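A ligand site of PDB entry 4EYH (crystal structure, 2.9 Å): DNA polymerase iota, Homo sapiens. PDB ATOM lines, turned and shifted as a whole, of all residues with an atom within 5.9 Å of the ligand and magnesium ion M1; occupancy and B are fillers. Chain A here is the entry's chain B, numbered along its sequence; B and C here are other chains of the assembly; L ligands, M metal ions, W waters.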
ATOM      1  N   ASP A  34     -20.289  13.546  25.631  1.00  0.00           N
ATOM      2  CA  ASP A  34     -19.502  14.747  25.464  1.00  0.00           C
ATOM      3  C   ASP A  34     -20.094  15.561  24.342  1.00  0.00           C
ATOM      4  O   ASP A  34     -20.133  15.110  23.210  1.00  0.00           O
ATOM      5  CB  ASP A  34     -18.089  14.335  25.051  1.00  0.00           C
ATOM      6  CG  ASP A  34     -17.019  15.251  25.619  1.00  0.00           C
ATOM      7  OD1 ASP A  34     -17.336  16.389  26.019  1.00  0.00           O
ATOM      8  OD2 ASP A  34     -15.850  14.829  25.632  1.00  0.00           O
ATOM      9  N   LEU A  35     -20.567  16.757  24.654  1.00  0.00           N
ATOM     10  CA  LEU A  35     -21.209  17.608  23.653  1.00  0.00           C
ATOM     11  C   LEU A  35     -20.203  18.358  22.806  1.00  0.00           C
ATOM     12  O   LEU A  35     -19.367  19.085  23.329  1.00  0.00           O
ATOM     13  CB  LEU A  35     -22.127  18.611  24.344  1.00  0.00           C
ATOM     14  CG  LEU A  35     -23.516  18.156  24.770  1.00  0.00           C
ATOM     15  CD1 LEU A  35     -24.535  18.947  23.996  1.00  0.00           C
ATOM     16  CD2 LEU A  35     -23.714  16.668  24.565  1.00  0.00           C
ATOM     17  N   ASP A  36     -20.287  18.202  21.492  1.00  0.00           N
ATOM     18  CA  ASP A  36     -19.392  18.904  20.588  1.00  0.00           C
ATOM     19  C   ASP A  36     -19.428  20.389  20.868  1.00  0.00           C
ATOM     20  O   ASP A  36     -20.515  20.954  21.015  1.00  0.00           O
ATOM     21  CB  ASP A  36     -19.805  18.682  19.140  1.00  0.00           C
ATOM     22  CG  ASP A  36     -19.721  17.239  18.717  1.00  0.00           C
ATOM     23  OD1 ASP A  36     -18.784  16.535  19.137  1.00  0.00           O
ATOM     24  OD2 ASP A  36     -20.587  16.815  17.924  1.00  0.00           O
ATOM     25  N   CYS A  37     -18.254  21.007  20.948  1.00  0.00           N
ATOM     26  CA  CYS A  37     -18.112  22.450  21.193  1.00  0.00           C
ATOM     27  C   CYS A  37     -19.348  23.066  21.828  1.00  0.00           C
ATOM     28  O   CYS A  37     -20.184  23.655  21.137  1.00  0.00           O
ATOM     29  CB  CYS A  37     -17.745  23.189  19.912  1.00  0.00           C
ATOM     30  SG  CYS A  37     -18.738  22.759  18.445  1.00  0.00           S
ATOM     31  N   PHE A  38     -19.453  22.959  23.147  1.00  0.00           N
ATOM     32  CA  PHE A  38     -20.704  23.258  23.825  1.00  0.00           C
ATOM     33  C   PHE A  38     -21.282  24.662  23.630  1.00  0.00           C
ATOM     34  O   PHE A  38     -22.370  24.815  23.073  1.00  0.00           O
ATOM     35  CB  PHE A  38     -20.606  22.947  25.315  1.00  0.00           C
ATOM     36  CG  PHE A  38     -21.921  23.008  26.020  1.00  0.00           C
ATOM     37  CD1 PHE A  38     -23.053  22.493  25.419  1.00  0.00           C
ATOM     38  CD2 PHE A  38     -22.037  23.580  27.272  1.00  0.00           C
ATOM     39  CE1 PHE A  38     -24.269  22.546  26.051  1.00  0.00           C
ATOM     40  CE2 PHE A  38     -23.258  23.628  27.916  1.00  0.00           C
ATOM     41  CZ  PHE A  38     -24.380  23.109  27.302  1.00  0.00           C
ATOM     42  N   TYR A  39     -20.569  25.672  24.101  1.00  0.00           N
ATOM     43  CA  TYR A  39     -21.050  27.044  24.002  1.00  0.00           C
ATOM     44  C   TYR A  39     -21.329  27.405  22.549  1.00  0.00           C
ATOM     45  O   TYR A  39     -22.338  28.039  22.228  1.00  0.00           O
ATOM     46  CB  TYR A  39     -20.051  28.021  24.602  1.00  0.00           C
ATOM     47  CG  TYR A  39     -19.703  27.750  26.052  1.00  0.00           C
ATOM     48  CD1 TYR A  39     -18.570  28.314  26.630  1.00  0.00           C
ATOM     49  CD2 TYR A  39     -20.509  26.950  26.846  1.00  0.00           C
ATOM     50  CE1 TYR A  39     -18.237  28.076  27.947  1.00  0.00           C
ATOM     51  CE2 TYR A  39     -20.193  26.703  28.169  1.00  0.00           C
ATOM     52  CZ  TYR A  39     -19.049  27.275  28.722  1.00  0.00           C
ATOM     53  OH  TYR A  39     -18.716  27.037  30.039  1.00  0.00           O
ATOM     54  N   ALA A  40     -20.431  26.971  21.661  1.00  0.00           N
ATOM     55  CA  ALA A  40     -20.581  27.170  20.223  1.00  0.00           C
ATOM     56  C   ALA A  40     -21.964  26.725  19.765  1.00  0.00           C
ATOM     57  O   ALA A  40     -22.696  27.492  19.141  1.00  0.00           O
ATOM     58  CB  ALA A  40     -19.507  26.410  19.476  1.00  0.00           C
ATOM     59  N   GLN A  59     -14.482  34.780  25.935  1.00  0.00           N
ATOM     60  CA  GLN A  59     -14.422  35.090  27.358  1.00  0.00           C
ATOM     61  C   GLN A  59     -13.267  36.048  27.510  1.00  0.00           C
ATOM     62  O   GLN A  59     -12.103  35.676  27.302  1.00  0.00           O
ATOM     63  CB  GLN A  59     -14.131  33.840  28.188  1.00  0.00           C
ATOM     64  CG  GLN A  59     -15.325  32.929  28.458  1.00  0.00           C
ATOM     65  CD  GLN A  59     -15.119  32.065  29.695  1.00  0.00           C
ATOM     66  OE1 GLN A  59     -14.141  32.258  30.447  1.00  0.00           O
ATOM     67  NE2 GLN A  59     -16.025  31.123  29.925  1.00  0.00           N
ATOM     68  N   VAL A  64     -12.736  30.654  23.940  1.00  0.00           N
ATOM     69  CA  VAL A  64     -12.647  29.432  24.739  1.00  0.00           C
ATOM     70  C   VAL A  64     -13.211  28.201  24.037  1.00  0.00           C
ATOM     71  O   VAL A  64     -12.930  27.063  24.415  1.00  0.00           O
ATOM     72  CB  VAL A  64     -13.302  29.606  26.112  1.00  0.00           C
ATOM     73  CG1 VAL A  64     -12.349  30.308  27.081  1.00  0.00           C
ATOM     74  CG2 VAL A  64     -14.620  30.376  25.971  1.00  0.00           C
ATOM     75  N   THR A  65     -14.002  28.431  23.004  1.00  0.00           N
ATOM     76  CA  THR A  65     -14.449  27.347  22.144  1.00  0.00           C
ATOM     77  C   THR A  65     -14.860  27.932  20.802  1.00  0.00           C
ATOM     78  O   THR A  65     -14.754  29.138  20.591  1.00  0.00           O
ATOM     79  CB  THR A  65     -15.604  26.551  22.787  1.00  0.00           C
ATOM     80  OG1 THR A  65     -15.756  25.296  22.110  1.00  0.00           O
ATOM     81  CG2 THR A  65     -16.912  27.336  22.737  1.00  0.00           C
ATOM     82  N   CYS A  66     -15.331  27.079  19.892  1.00  0.00           N
ATOM     83  CA  CYS A  66     -15.718  27.508  18.545  1.00  0.00           C
ATOM     84  C   CYS A  66     -16.200  26.338  17.689  1.00  0.00           C
ATOM     85  O   CYS A  66     -15.677  25.222  17.799  1.00  0.00           O
ATOM     86  CB  CYS A  66     -14.535  28.201  17.853  1.00  0.00           C
ATOM     87  SG  CYS A  66     -12.988  27.259  17.936  1.00  0.00           S
ATOM     88  N   TYR A  68     -17.021  23.786  14.505  1.00  0.00           N
ATOM     89  CA  TYR A  68     -16.072  23.067  13.661  1.00  0.00           C
ATOM     90  C   TYR A  68     -15.817  23.780  12.321  1.00  0.00           C
ATOM     91  O   TYR A  68     -14.693  23.755  11.813  1.00  0.00           O
ATOM     92  CB  TYR A  68     -16.509  21.602  13.490  1.00  0.00           C
ATOM     93  CG  TYR A  68     -16.202  20.757  14.704  1.00  0.00           C
ATOM     94  CD1 TYR A  68     -17.078  20.695  15.776  1.00  0.00           C
ATOM     95  CD2 TYR A  68     -15.004  20.056  14.809  1.00  0.00           C
ATOM     96  CE1 TYR A  68     -16.780  19.947  16.906  1.00  0.00           C
ATOM     97  CE2 TYR A  68     -14.696  19.304  15.926  1.00  0.00           C
ATOM     98  CZ  TYR A  68     -15.590  19.258  16.971  1.00  0.00           C
ATOM     99  OH  TYR A  68     -15.287  18.493  18.090  1.00  0.00           O
ATOM    100  N   ARG A  71     -13.102  25.806  13.048  1.00  0.00           N
ATOM    101  CA  ARG A  71     -11.887  25.079  13.410  1.00  0.00           C
ATOM    102  C   ARG A  71     -11.052  24.865  12.159  1.00  0.00           C
ATOM    103  O   ARG A  71      -9.825  24.803  12.218  1.00  0.00           O
ATOM    104  CB  ARG A  71     -12.208  23.744  14.114  1.00  0.00           C
ATOM    105  CG  ARG A  71     -12.448  23.884  15.606  1.00  0.00           C
ATOM    106  CD  ARG A  71     -11.920  22.700  16.400  1.00  0.00           C
ATOM    107  NE  ARG A  71     -12.094  22.903  17.838  1.00  0.00           N
ATOM    108  CZ  ARG A  71     -13.206  22.596  18.518  1.00  0.00           C
ATOM    109  NH1 ARG A  71     -14.257  22.055  17.903  1.00  0.00           N
ATOM    110  NH2 ARG A  71     -13.267  22.838  19.825  1.00  0.00           N
ATOM    111  N   LYS A  77      -9.092  25.730  20.261  1.00  0.00           N
ATOM    112  CA  LYS A  77      -9.599  25.970  21.615  1.00  0.00           C
ATOM    113  C   LYS A  77      -8.631  26.822  22.450  1.00  0.00           C
ATOM    114  O   LYS A  77      -7.409  26.689  22.343  1.00  0.00           O
ATOM    115  CB  LYS A  77      -9.881  24.641  22.338  1.00  0.00           C
ATOM    116  CG  LYS A  77     -11.281  24.097  22.129  1.00  0.00           C
ATOM    117  CD  LYS A  77     -11.672  23.104  23.214  1.00  0.00           C
ATOM    118  CE  LYS A  77     -10.647  21.984  23.363  1.00  0.00           C
ATOM    119  NZ  LYS A  77     -11.266  20.693  23.815  1.00  0.00           N
ATOM    120  N   LEU A  78      -9.187  27.704  23.280  1.00  0.00           N
ATOM    121  CA  LEU A  78      -8.406  28.567  24.174  1.00  0.00           C
ATOM    122  C   LEU A  78      -7.330  29.414  23.449  1.00  0.00           C
ATOM    123  O   LEU A  78      -6.194  29.541  23.932  1.00  0.00           O
ATOM    124  CB  LEU A  78      -7.785  27.740  25.329  1.00  0.00           C
ATOM    125  CG  LEU A  78      -8.673  27.146  26.459  1.00  0.00           C
ATOM    126  CD1 LEU A  78      -7.980  26.001  27.241  1.00  0.00           C
ATOM    127  CD2 LEU A  78      -9.182  28.198  27.458  1.00  0.00           C
ATOM    128  N   ASP A 126     -20.708  20.173  29.975  1.00  0.00           N
ATOM    129  CA  ASP A 126     -20.992  19.483  28.717  1.00  0.00           C
ATOM    130  C   ASP A 126     -20.629  17.999  28.710  1.00  0.00           C
ATOM    131  O   ASP A 126     -20.578  17.381  27.648  1.00  0.00           O
ATOM    132  CB  ASP A 126     -20.263  20.159  27.563  1.00  0.00           C
ATOM    133  CG  ASP A 126     -18.764  19.900  27.581  1.00  0.00           C
ATOM    134  OD1 ASP A 126     -18.232  19.460  26.548  1.00  0.00           O
ATOM    135  OD2 ASP A 126     -18.133  20.150  28.632  1.00  0.00           O
ATOM    136  N   GLU A 127     -20.389  17.430  29.887  1.00  0.00           N
ATOM    137  CA  GLU A 127     -20.022  16.030  30.023  1.00  0.00           C
ATOM    138  C   GLU A 127     -20.928  15.290  31.005  1.00  0.00           C
ATOM    139  O   GLU A 127     -21.252  15.818  32.063  1.00  0.00           O
ATOM    140  CB  GLU A 127     -18.563  15.877  30.451  1.00  0.00           C
ATOM    141  CG  GLU A 127     -17.535  16.359  29.415  1.00  0.00           C
ATOM    142  CD  GLU A 127     -16.147  15.798  29.676  1.00  0.00           C
ATOM    143  OE1 GLU A 127     -15.997  15.072  30.685  1.00  0.00           O
ATOM    144  OE2 GLU A 127     -15.220  16.073  28.887  1.00  0.00           O
ATOM    145  N   CYS A 196     -20.654  13.220  21.217  1.00  0.00           N
ATOM    146  CA  CYS A 196     -19.958  11.947  21.129  1.00  0.00           C
ATOM    147  C   CYS A 196     -20.251  11.097  22.347  1.00  0.00           C
ATOM    148  O   CYS A 196     -20.606  11.598  23.405  1.00  0.00           O
ATOM    149  CB  CYS A 196     -18.459  12.178  21.019  1.00  0.00           C
ATOM    150  SG  CYS A 196     -18.017  13.243  19.674  1.00  0.00           S
ATOM    151  N   LYS A 214     -14.407  12.233  16.709  1.00  0.00           N
ATOM    152  CA  LYS A 214     -15.141  13.480  16.852  1.00  0.00           C
ATOM    153  C   LYS A 214     -15.315  14.109  15.474  1.00  0.00           C
ATOM    154  O   LYS A 214     -14.575  13.792  14.550  1.00  0.00           O
ATOM    155  CB  LYS A 214     -14.409  14.436  17.791  1.00  0.00           C
ATOM    156  CG  LYS A 214     -14.024  13.806  19.122  1.00  0.00           C
ATOM    157  CD  LYS A 214     -14.043  14.811  20.270  1.00  0.00           C
ATOM    158  CE  LYS A 214     -13.059  15.961  20.041  1.00  0.00           C
ATOM    159  NZ  LYS A 214     -13.093  16.952  21.152  1.00  0.00           N
ATOM    160  N   PRO A 215     -16.324  14.987  15.336  1.00  0.00           N
ATOM    161  CA  PRO A 215     -17.351  15.229  16.343  1.00  0.00           C
ATOM    162  C   PRO A 215     -18.612  14.435  16.001  1.00  0.00           C
ATOM    163  O   PRO A 215     -18.670  13.828  14.953  1.00  0.00           O
ATOM    164  CB  PRO A 215     -17.607  16.720  16.190  1.00  0.00           C
ATOM    165  CG  PRO A 215     -17.420  16.965  14.736  1.00  0.00           C
ATOM    166  CD  PRO A 215     -16.355  16.005  14.270  1.00  0.00           C
ATOM    167  P   DG8 B   1      -4.726  36.230  35.318  1.00  0.00           P
ATOM    168  O1P DG8 B   1      -5.658  37.425  35.284  1.00  0.00           O
ATOM    169  O2P DG8 B   1      -3.562  36.085  34.348  1.00  0.00           O
ATOM    170  O5' DG8 B   1      -5.623  34.885  35.313  1.00  0.00           O
ATOM    171  C5' DG8 B   1      -6.948  34.885  35.855  1.00  0.00           C
ATOM    172  C4' DG8 B   1      -7.909  34.596  34.711  1.00  0.00           C
ATOM    173  C3' DG8 B   1      -9.312  34.108  35.079  1.00  0.00           C
ATOM    174  C2' DG8 B   1      -9.675  33.146  33.959  1.00  0.00           C
ATOM    175  C1' DG8 B   1      -8.361  32.812  33.271  1.00  0.00           C
ATOM    176  O4' DG8 B   1      -7.316  33.611  33.861  1.00  0.00           O
ATOM    177  N9  DG8 B   1      -8.143  31.347  33.426  1.00  0.00           N
ATOM    178  C8  DG8 B   1      -7.111  30.665  34.024  1.00  0.00           C
ATOM    179  N7  DG8 B   1      -7.287  29.332  33.924  1.00  0.00           N
ATOM    180  C5  DG8 B   1      -8.452  29.150  33.232  1.00  0.00           C
ATOM    181  C6  DG8 B   1      -9.153  28.025  32.823  1.00  0.00           C
ATOM    182  O6  DG8 B   1      -8.684  26.893  33.099  1.00  0.00           O
ATOM    183  N1  DG8 B   1     -10.340  28.161  32.119  1.00  0.00           N
ATOM    184  C2  DG8 B   1     -10.833  29.408  31.816  1.00  0.00           C
ATOM    185  N2  DG8 B   1     -12.051  29.587  31.090  1.00  0.00           N
ATOM    186  N3  DG8 B   1     -10.156  30.510  32.223  1.00  0.00           N
ATOM    187  C4  DG8 B   1      -8.988  30.401  32.912  1.00  0.00           C
ATOM    188  N24 DG8 B   1      -5.981  31.369  34.715  1.00  0.00           N
ATOM    189  C25 DG8 B   1      -5.087  30.547  35.593  1.00  0.00           C
ATOM    190  C30 DG8 B   1      -4.205  31.206  36.460  1.00  0.00           C
ATOM    191  C35 DG8 B   1      -3.339  30.467  37.282  1.00  0.00           C
ATOM    192  C34 DG8 B   1      -2.469  31.143  38.141  1.00  0.00           C
ATOM    193  C38 DG8 B   1      -1.616  30.408  38.967  1.00  0.00           C
ATOM    194  C37 DG8 B   1      -1.623  29.007  38.909  1.00  0.00           C
ATOM    195  C36 DG8 B   1      -2.485  28.336  38.046  1.00  0.00           C
ATOM    196  C28 DG8 B   1      -3.346  29.065  37.223  1.00  0.00           C
ATOM    197  C27 DG8 B   1      -4.219  28.412  36.354  1.00  0.00           C
ATOM    198  C26 DG8 B   1      -5.073  29.155  35.539  1.00  0.00           C
ATOM    199  C39 DG8 B   1      -0.750  31.071  39.828  1.00  0.00           C
ATOM    200  C40 DG8 B   1      -0.751  32.458  39.878  1.00  0.00           C
ATOM    201  C41 DG8 B   1      -1.605  33.202  39.063  1.00  0.00           C
ATOM    202  C33 DG8 B   1      -2.461  32.535  38.189  1.00  0.00           C
ATOM    203  C32 DG8 B   1      -3.323  33.274  37.376  1.00  0.00           C
ATOM    204  C31 DG8 B   1      -4.194  32.598  36.517  1.00  0.00           C
ATOM    205  O3' DG8 B   1     -10.267  35.178  35.056  1.00  0.00           O
ATOM    206  P    DG B   2     -11.813  34.907  35.455  1.00  0.00           P
ATOM    207  OP1  DG B   2     -12.353  36.169  36.029  1.00  0.00           O
ATOM    208  OP2  DG B   2     -11.853  33.651  36.276  1.00  0.00           O
ATOM    209  O5'  DG B   2     -12.547  34.657  34.026  1.00  0.00           O
ATOM    210  C5'  DG B   2     -13.960  34.517  33.864  1.00  0.00           C
ATOM    211  C4'  DG B   2     -14.555  33.119  34.111  1.00  0.00           C
ATOM    212  O4'  DG B   2     -13.549  32.053  34.044  1.00  0.00           O
ATOM    213  C3'  DG B   2     -15.228  32.958  35.487  1.00  0.00           C
ATOM    214  O3'  DG B   2     -16.486  32.250  35.436  1.00  0.00           O
ATOM    215  C2'  DG B   2     -14.198  32.159  36.278  1.00  0.00           C
ATOM    216  C1'  DG B   2     -13.813  31.210  35.148  1.00  0.00           C
ATOM    217  N9   DG B   2     -12.684  30.374  35.499  1.00  0.00           N
ATOM    218  C8   DG B   2     -11.535  30.658  36.204  1.00  0.00           C
ATOM    219  N7   DG B   2     -10.753  29.610  36.346  1.00  0.00           N
ATOM    220  C5   DG B   2     -11.451  28.597  35.702  1.00  0.00           C
ATOM    221  C6   DG B   2     -11.153  27.229  35.513  1.00  0.00           C
ATOM    222  O6   DG B   2     -10.135  26.615  35.894  1.00  0.00           O
ATOM    223  N1   DG B   2     -12.167  26.563  34.805  1.00  0.00           N
ATOM    224  C2   DG B   2     -13.331  27.151  34.335  1.00  0.00           C
ATOM    225  N2   DG B   2     -14.200  26.380  33.678  1.00  0.00           N
ATOM    226  N3   DG B   2     -13.618  28.424  34.512  1.00  0.00           N
ATOM    227  C4   DG B   2     -12.641  29.053  35.191  1.00  0.00           C
ATOM    228  P    DC C   7     -11.006  17.284  31.747  1.00  0.00           P
ATOM    229  OP1  DC C   7     -10.704  16.242  30.751  1.00  0.00           O
ATOM    230  OP2  DC C   7      -9.969  18.246  32.189  1.00  0.00           O
ATOM    231  O5'  DC C   7     -12.225  18.188  31.235  1.00  0.00           O
ATOM    232  C5'  DC C   7     -13.575  17.893  31.613  1.00  0.00           C
ATOM    233  C4'  DC C   7     -14.396  19.136  31.385  1.00  0.00           C
ATOM    234  O4'  DC C   7     -14.425  19.972  32.582  1.00  0.00           O
ATOM    235  C3'  DC C   7     -13.753  20.014  30.337  1.00  0.00           C
ATOM    236  O3'  DC C   7     -14.146  19.576  29.055  1.00  0.00           O
ATOM    237  C2'  DC C   7     -14.274  21.407  30.681  1.00  0.00           C
ATOM    238  C1'  DC C   7     -14.391  21.343  32.212  1.00  0.00           C
ATOM    239  N1   DC C   7     -13.258  22.070  32.912  1.00  0.00           N
ATOM    240  C2   DC C   7     -13.430  23.378  33.419  1.00  0.00           C
ATOM    241  O2   DC C   7     -14.520  23.952  33.325  1.00  0.00           O
ATOM    242  N3   DC C   7     -12.376  23.977  34.032  1.00  0.00           N
ATOM    243  C4   DC C   7     -11.220  23.333  34.138  1.00  0.00           C
ATOM    244  N4   DC C   7     -10.216  23.962  34.756  1.00  0.00           N
ATOM    245  C5   DC C   7     -11.011  22.021  33.630  1.00  0.00           C
ATOM    246  C6   DC C   7     -12.051  21.428  33.033  1.00  0.00           C
HETATM  247  N1  LIG L   1     -13.617  25.805  29.353  1.00  0.00           N
HETATM  248  C1  LIG L   1     -13.184  26.804  30.209  1.00  0.00           C
HETATM  249  N2  LIG L   1     -12.016  26.646  30.930  1.00  0.00           N
HETATM  250  C2  LIG L   1     -11.217  25.538  30.742  1.00  0.00           C
HETATM  251  C3  LIG L   1     -11.654  24.526  29.888  1.00  0.00           C
HETATM  252  C4  LIG L   1     -12.790  24.745  29.082  1.00  0.00           C
HETATM  253  O1  LIG L   1     -13.849  27.832  30.314  1.00  0.00           O
HETATM  254  N3  LIG L   1     -10.051  25.436  31.367  1.00  0.00           N
HETATM  255  C5  LIG L   1     -14.973  25.931  28.767  1.00  0.00           C
HETATM  256  C6  LIG L   1     -14.938  25.974  27.242  1.00  0.00           C
HETATM  257  C7  LIG L   1     -15.850  24.853  26.775  1.00  0.00           C
HETATM  258  C8  LIG L   1     -16.334  24.170  28.050  1.00  0.00           C
HETATM  259  O2  LIG L   1     -15.768  24.828  29.176  1.00  0.00           O
HETATM  260  O3  LIG L   1     -16.976  25.325  26.054  1.00  0.00           O
HETATM  261  C9  LIG L   1     -15.955  22.688  28.091  1.00  0.00           C
HETATM  262  O4  LIG L   1     -14.690  22.418  27.501  1.00  0.00           O
HETATM  263  P1  LIG L   1     -14.447  21.112  26.572  1.00  0.00           P
HETATM  264  O5  LIG L   1     -15.518  20.070  26.858  1.00  0.00           O
HETATM  265  O6  LIG L   1     -13.083  20.506  26.831  1.00  0.00           O
HETATM  266  O7  LIG L   1     -14.608  21.591  25.025  1.00  0.00           O
HETATM  267  P2  LIG L   1     -15.838  21.344  23.998  1.00  0.00           P
HETATM  268  O8  LIG L   1     -16.573  22.668  23.982  1.00  0.00           O
HETATM  269  O9  LIG L   1     -16.745  20.193  24.349  1.00  0.00           O
HETATM  270  O10 LIG L   1     -15.067  21.188  22.577  1.00  0.00           O
HETATM  271  P3  LIG L   1     -14.831  19.904  21.629  1.00  0.00           P
HETATM  272  O11 LIG L   1     -15.698  20.022  20.402  1.00  0.00           O
HETATM  273  O12 LIG L   1     -13.408  19.916  21.118  1.00  0.00           O
HETATM  274  O13 LIG L   1     -15.105  18.616  22.410  1.00  0.00           O
HETATM  275 MG    MG M   1     -17.017  17.344  23.456  1.00  0.00          MG
HETATM  276 MG    MG M   2     -14.660  17.434  26.709  1.00  0.00          MG
HETATM  277  O   HOH W   1     -17.084  16.154  20.869  1.00  0.00           O
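N2 of DG8 1 of chain B lies close to the side-chain amide oxygen (OE1) of Gln 59, at 3.5 Å.
N2 of DG 2 of chain B lies close to O2 of DC 7 of chain C, at 2.5 Å.
N of Leu 35 lies within hydrogen-bond range of O of Asp 126 (3.1 Å).
The backbone carbonyl oxygen (O) of Asp 34 is in hydrogen-bond range of the backbone NH (N) of Cys 196.
NH1 of Arg 71 lies within hydrogen-bond range of O of Cys 66, at 3.5 Å.
The side-chain carboxylate (OD1) of Asp 36 is in hydrogen-bond range of the side-chain sulfur (SG) of Cys 196 (3.4 Å).
Asp 36 touches the ligand.
Tyr 39 touches the ligand.
NE2 of Gln 59 touches O1 of the ligand, at 3.96 Å.
Val 64 touches the ligand (O to C6, 3.6 Å).
DG 2 of chain B touches the ligand (N2 to N2, 3.5 Å).
Hydrophobic or aromatic side chains within 4 Å of the ligand: Tyr 39 and Tyr 68.
16 residues have an atom within 4 Å of the ligand: Leu 35, Asp 36, Cys 37, Phe 38, Tyr 39, Gln 59, Val 64, Thr 65, Tyr 68, Arg 71, Lys 77, Asp 126, Lys 214, DG8 1 of chain B, DG 2 of chain B and DC 7 of chain C.
Magnesium ion M1 is bound by O13 of the ligand (2.5 Å).
Slightly farther from magnesium ion M1 lies OD1 of Asp 34 (2.8 Å).
Slightly farther from magnesium ion M1 lies water W1 (2.8 Å).
O6 of DG8 1 of chain B is in hydrogen-bond range of a nitrogen (N3) of the ligand, 2.6 Å away.
O3' of DC 7 of chain C lies close to an oxygen (O6) of the ligand (2.6 Å).
O9 of the ligand sits close to OD1 of Asp 126, 2.8 Å away.
N of Cys 37 lies within hydrogen-bond range of O11 of the ligand (2.8 Å).
The side-chain hydroxyl of Tyr 68 sits at hydrogen-bond distance from an oxygen (O11) of the ligand, 2.8 Å away.
The side-chain amino group of Lys 214 is in salt-bridge range of an oxygen (O12) of the ligand.
The backbone carbonyl oxygen (O) of Leu 35 sits close to an oxygen (O9) of the ligand (3.0 Å).
O8 of the ligand is in hydrogen-bond range of N of Phe 38 (3.0 Å).
An oxygen (O12) of the ligand is in salt-bridge range of the guanidinium group (NH2) of Arg 71 (3.2 Å).
OG1 of Thr 65 sits at hydrogen-bond distance from O8 of the ligand.
The side-chain amino group of Lys 77 lies within salt-bridge range of an oxygen (O6) of the ligand, 3.5 Å away.
Water W1 lies within hydrogen-bond range of OD1 of Asp 36 (2.5 Å) and SG of Cys 196 (3.3 Å).
Leu 35 touches magnesium ion M1 (O to MG, 2.9 Å).
N of Asp 36 touches magnesium ion M1, 3.9 Å away.
Asp 126 touches magnesium ion M1 (OD1 to MG, 3.9 Å).
The nearest printed residue that does not touch magnesium ion M1 is Lys 214 (4.6 Å).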
